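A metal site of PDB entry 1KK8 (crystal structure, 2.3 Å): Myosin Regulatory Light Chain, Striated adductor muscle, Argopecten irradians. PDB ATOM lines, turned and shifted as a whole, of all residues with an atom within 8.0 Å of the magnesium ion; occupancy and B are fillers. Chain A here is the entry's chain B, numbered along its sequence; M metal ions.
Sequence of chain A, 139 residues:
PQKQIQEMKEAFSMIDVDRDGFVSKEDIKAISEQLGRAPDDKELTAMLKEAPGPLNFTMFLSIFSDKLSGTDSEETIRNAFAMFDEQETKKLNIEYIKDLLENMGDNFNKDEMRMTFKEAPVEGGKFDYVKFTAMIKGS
The backbone carbonyl oxygen (O) of Phe 22 is bound to the magnesium ion (1.8 Å). The side-chain carboxylate (OD1) of Asp 20 is bound to the magnesium ion (2.0 Å). OD1 of Asp 16 binds the magnesium ion (2.2 Å). OD2 of Asp 27 is bound to the magnesium ion, at 2.4 Å. Slightly farther from the magnesium ion lies the side-chain carboxylate (OD1) of Asp 18 (2.8 Å).
The side-chain carboxylate of Asp 27 sits at hydrogen-bond distance from the backbone NH of Val 17. N of Gly 21 sits at hydrogen-bond distance from OD2 of Asp 16 (2.9 Å). The backbone NH (N) of Val 23 lies within hydrogen-bond range of the backbone carbonyl oxygen (O) of Leu 55, 2.9 Å away. The backbone NH (N) of Asp 18 sits at hydrogen-bond distance from the side-chain carboxylate (OD1) of Asp 27 (3.3 Å). The backbone NH (N) of Asp 27 lies close to the side-chain hydroxyl (OG) of Ser 24, at 3.4 Å. N of Asp 20 sits close to OD1 of Asp 18, at 3.3 Å.
N of Val 23 touches the magnesium ion, at 3.99 Å. Within 4 Å of the magnesium ion: Asp 16, Asp 18, Asp 20, Phe 22, Val 23 and Asp 27.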
ATOM      1  N   PHE A  12      15.621  22.746  15.392  1.00  0.00           N
ATOM      2  CA  PHE A  12      15.911  21.408  15.862  1.00  0.00           C
ATOM      3  C   PHE A  12      17.404  21.137  16.032  1.00  0.00           C
ATOM      4  O   PHE A  12      17.812  20.449  16.966  1.00  0.00           O
ATOM      5  CB  PHE A  12      15.321  20.354  14.930  1.00  0.00           C
ATOM      6  CG  PHE A  12      15.750  18.960  15.277  1.00  0.00           C
ATOM      7  CD1 PHE A  12      16.974  18.456  14.838  1.00  0.00           C
ATOM      8  CD2 PHE A  12      14.945  18.154  16.087  1.00  0.00           C
ATOM      9  CE1 PHE A  12      17.383  17.190  15.203  1.00  0.00           C
ATOM     10  CE2 PHE A  12      15.355  16.870  16.462  1.00  0.00           C
ATOM     11  CZ  PHE A  12      16.569  16.393  16.028  1.00  0.00           C
ATOM     12  N   ILE A  15      18.736  22.954  19.215  1.00  0.00           N
ATOM     13  CA  ILE A  15      18.341  22.375  20.496  1.00  0.00           C
ATOM     14  C   ILE A  15      19.200  21.136  20.731  1.00  0.00           C
ATOM     15  O   ILE A  15      19.589  20.837  21.864  1.00  0.00           O
ATOM     16  CB  ILE A  15      16.854  22.007  20.469  1.00  0.00           C
ATOM     17  CG1 ILE A  15      16.049  23.299  20.258  1.00  0.00           C
ATOM     18  CG2 ILE A  15      16.459  21.275  21.749  1.00  0.00           C
ATOM     19  CD1 ILE A  15      14.613  23.071  19.898  1.00  0.00           C
ATOM     20  N   ASP A  16      19.489  20.421  19.643  1.00  0.00           N
ATOM     21  CA  ASP A  16      20.337  19.220  19.671  1.00  0.00           C
ATOM     22  C   ASP A  16      21.766  19.744  19.768  1.00  0.00           C
ATOM     23  O   ASP A  16      22.429  19.951  18.757  1.00  0.00           O
ATOM     24  CB  ASP A  16      20.117  18.434  18.376  1.00  0.00           C
ATOM     25  CG  ASP A  16      21.037  17.240  18.236  1.00  0.00           C
ATOM     26  OD1 ASP A  16      21.287  16.542  19.244  1.00  0.00           O
ATOM     27  OD2 ASP A  16      21.500  16.996  17.097  1.00  0.00           O
ATOM     28  N   VAL A  17      22.222  19.940  20.996  1.00  0.00           N
ATOM     29  CA  VAL A  17      23.551  20.478  21.260  1.00  0.00           C
ATOM     30  C   VAL A  17      24.717  19.560  20.876  1.00  0.00           C
ATOM     31  O   VAL A  17      25.616  19.963  20.146  1.00  0.00           O
ATOM     32  CB  VAL A  17      23.687  20.891  22.738  1.00  0.00           C
ATOM     33  CG1 VAL A  17      25.013  21.604  22.964  1.00  0.00           C
ATOM     34  CG2 VAL A  17      22.522  21.783  23.138  1.00  0.00           C
ATOM     35  N   ASP A  18      24.692  18.325  21.371  1.00  0.00           N
ATOM     36  CA  ASP A  18      25.759  17.378  21.065  1.00  0.00           C
ATOM     37  C   ASP A  18      25.787  17.027  19.576  1.00  0.00           C
ATOM     38  O   ASP A  18      26.606  16.232  19.138  1.00  0.00           O
ATOM     39  CB  ASP A  18      25.617  16.100  21.905  1.00  0.00           C
ATOM     40  CG  ASP A  18      24.342  15.315  21.596  1.00  0.00           C
ATOM     41  OD1 ASP A  18      24.049  15.088  20.398  1.00  0.00           O
ATOM     42  OD2 ASP A  18      23.650  14.924  22.557  1.00  0.00           O
ATOM     43  N   ARG A  19      24.884  17.638  18.814  1.00  0.00           N
ATOM     44  CA  ARG A  19      24.794  17.403  17.373  1.00  0.00           C
ATOM     45  C   ARG A  19      24.903  15.916  17.054  1.00  0.00           C
ATOM     46  O   ARG A  19      25.991  15.408  16.774  1.00  0.00           O
ATOM     47  CB  ARG A  19      25.899  18.179  16.641  1.00  0.00           C
ATOM     48  N   ASP A  20      23.772  15.220  17.090  1.00  0.00           N
ATOM     49  CA  ASP A  20      23.773  13.794  16.805  1.00  0.00           C
ATOM     50  C   ASP A  20      22.463  13.359  16.148  1.00  0.00           C
ATOM     51  O   ASP A  20      22.277  12.188  15.819  1.00  0.00           O
ATOM     52  CB  ASP A  20      23.994  13.012  18.101  1.00  0.00           C
ATOM     53  CG  ASP A  20      22.747  12.925  18.958  1.00  0.00           C
ATOM     54  OD1 ASP A  20      22.143  13.971  19.252  1.00  0.00           O
ATOM     55  OD2 ASP A  20      22.374  11.788  19.338  1.00  0.00           O
ATOM     56  N   GLY A  21      21.556  14.318  15.959  1.00  0.00           N
ATOM     57  CA  GLY A  21      20.281  14.016  15.346  1.00  0.00           C
ATOM     58  C   GLY A  21      19.186  13.603  16.307  1.00  0.00           C
ATOM     59  O   GLY A  21      18.101  13.201  15.879  1.00  0.00           O
ATOM     60  N   PHE A  22      19.447  13.691  17.607  1.00  0.00           N
ATOM     61  CA  PHE A  22      18.460  13.326  18.599  1.00  0.00           C
ATOM     62  C   PHE A  22      18.492  14.267  19.780  1.00  0.00           C
ATOM     63  O   PHE A  22      19.540  14.490  20.381  1.00  0.00           O
ATOM     64  CB  PHE A  22      18.678  11.903  19.091  1.00  0.00           C
ATOM     65  CG  PHE A  22      18.419  10.857  18.066  1.00  0.00           C
ATOM     66  CD1 PHE A  22      19.354  10.594  17.065  1.00  0.00           C
ATOM     67  CD2 PHE A  22      17.229  10.130  18.075  1.00  0.00           C
ATOM     68  CE1 PHE A  22      19.109   9.626  16.090  1.00  0.00           C
ATOM     69  CE2 PHE A  22      16.957   9.174  17.104  1.00  0.00           C
ATOM     70  CZ  PHE A  22      17.911   8.916  16.110  1.00  0.00           C
ATOM     71  N   VAL A  23      17.329  14.823  20.107  1.00  0.00           N
ATOM     72  CA  VAL A  23      17.211  15.736  21.236  1.00  0.00           C
ATOM     73  C   VAL A  23      17.006  14.928  22.509  1.00  0.00           C
ATOM     74  O   VAL A  23      16.014  14.222  22.651  1.00  0.00           O
ATOM     75  CB  VAL A  23      16.013  16.696  21.056  1.00  0.00           C
ATOM     76  CG1 VAL A  23      15.835  17.540  22.308  1.00  0.00           C
ATOM     77  CG2 VAL A  23      16.218  17.585  19.839  1.00  0.00           C
ATOM     78  N   SER A  24      17.970  15.025  23.431  1.00  0.00           N
ATOM     79  CA  SER A  24      17.888  14.301  24.696  1.00  0.00           C
ATOM     80  C   SER A  24      17.667  15.262  25.857  1.00  0.00           C
ATOM     81  O   SER A  24      17.663  16.481  25.686  1.00  0.00           O
ATOM     82  CB  SER A  24      19.174  13.497  24.935  1.00  0.00           C
ATOM     83  OG  SER A  24      20.301  14.345  25.090  1.00  0.00           O
ATOM     84  N   LYS A  25      17.492  14.697  27.044  1.00  0.00           N
ATOM     85  CA  LYS A  25      17.270  15.470  28.262  1.00  0.00           C
ATOM     86  C   LYS A  25      18.406  16.490  28.411  1.00  0.00           C
ATOM     87  O   LYS A  25      18.167  17.670  28.660  1.00  0.00           O
ATOM     88  CB  LYS A  25      17.231  14.522  29.463  1.00  0.00           C
ATOM     89  CG  LYS A  25      16.613  15.105  30.730  1.00  0.00           C
ATOM     90  CD  LYS A  25      16.411  14.031  31.815  1.00  0.00           C
ATOM     91  CE  LYS A  25      15.441  12.950  31.356  1.00  0.00           C
ATOM     92  NZ  LYS A  25      15.319  11.801  32.311  1.00  0.00           N
ATOM     93  N   GLU A  26      19.634  16.021  28.260  1.00  0.00           N
ATOM     94  CA  GLU A  26      20.817  16.861  28.361  1.00  0.00           C
ATOM     95  C   GLU A  26      20.862  17.900  27.251  1.00  0.00           C
ATOM     96  O   GLU A  26      21.358  19.008  27.450  1.00  0.00           O
ATOM     97  CB  GLU A  26      22.069  15.995  28.324  1.00  0.00           C
ATOM     98  CG  GLU A  26      22.191  15.066  29.524  1.00  0.00           C
ATOM     99  CD  GLU A  26      20.915  14.262  29.761  1.00  0.00           C
ATOM    100  OE1 GLU A  26      20.549  13.455  28.870  1.00  0.00           O
ATOM    101  OE2 GLU A  26      20.284  14.461  30.822  1.00  0.00           O
ATOM    102  N   ASP A  27      20.341  17.546  26.079  1.00  0.00           N
ATOM    103  CA  ASP A  27      20.312  18.477  24.953  1.00  0.00           C
ATOM    104  C   ASP A  27      19.460  19.690  25.310  1.00  0.00           C
ATOM    105  O   ASP A  27      19.814  20.835  25.005  1.00  0.00           O
ATOM    106  CB  ASP A  27      19.729  17.801  23.717  1.00  0.00           C
ATOM    107  CG  ASP A  27      20.697  16.880  23.037  1.00  0.00           C
ATOM    108  OD1 ASP A  27      21.761  17.374  22.598  1.00  0.00           O
ATOM    109  OD2 ASP A  27      20.401  15.677  22.935  1.00  0.00           O
ATOM    110  N   ILE A  28      18.324  19.419  25.951  1.00  0.00           N
ATOM    111  CA  ILE A  28      17.390  20.460  26.363  1.00  0.00           C
ATOM    112  C   ILE A  28      17.902  21.232  27.569  1.00  0.00           C
ATOM    113  O   ILE A  28      17.901  22.469  27.581  1.00  0.00           O
ATOM    114  CB  ILE A  28      16.022  19.839  26.737  1.00  0.00           C
ATOM    115  CG1 ILE A  28      15.428  19.114  25.537  1.00  0.00           C
ATOM    116  CG2 ILE A  28      15.075  20.926  27.205  1.00  0.00           C
ATOM    117  CD1 ILE A  28      14.239  18.287  25.884  1.00  0.00           C
ATOM    118  N   LEU A  55      13.933  10.989  20.060  1.00  0.00           N
ATOM    119  CA  LEU A  55      13.512  12.222  19.428  1.00  0.00           C
ATOM    120  C   LEU A  55      14.362  12.788  18.297  1.00  0.00           C
ATOM    121  O   LEU A  55      15.307  13.555  18.528  1.00  0.00           O
ATOM    122  CB  LEU A  55      13.303  13.296  20.504  1.00  0.00           C
ATOM    123  CG  LEU A  55      12.968  14.697  19.986  1.00  0.00           C
ATOM    124  CD1 LEU A  55      11.703  14.650  19.155  1.00  0.00           C
ATOM    125  CD2 LEU A  55      12.819  15.647  21.141  1.00  0.00           C
HETATM  126 MG    MG M   1      21.257  15.002  20.779  1.00  0.00          MG
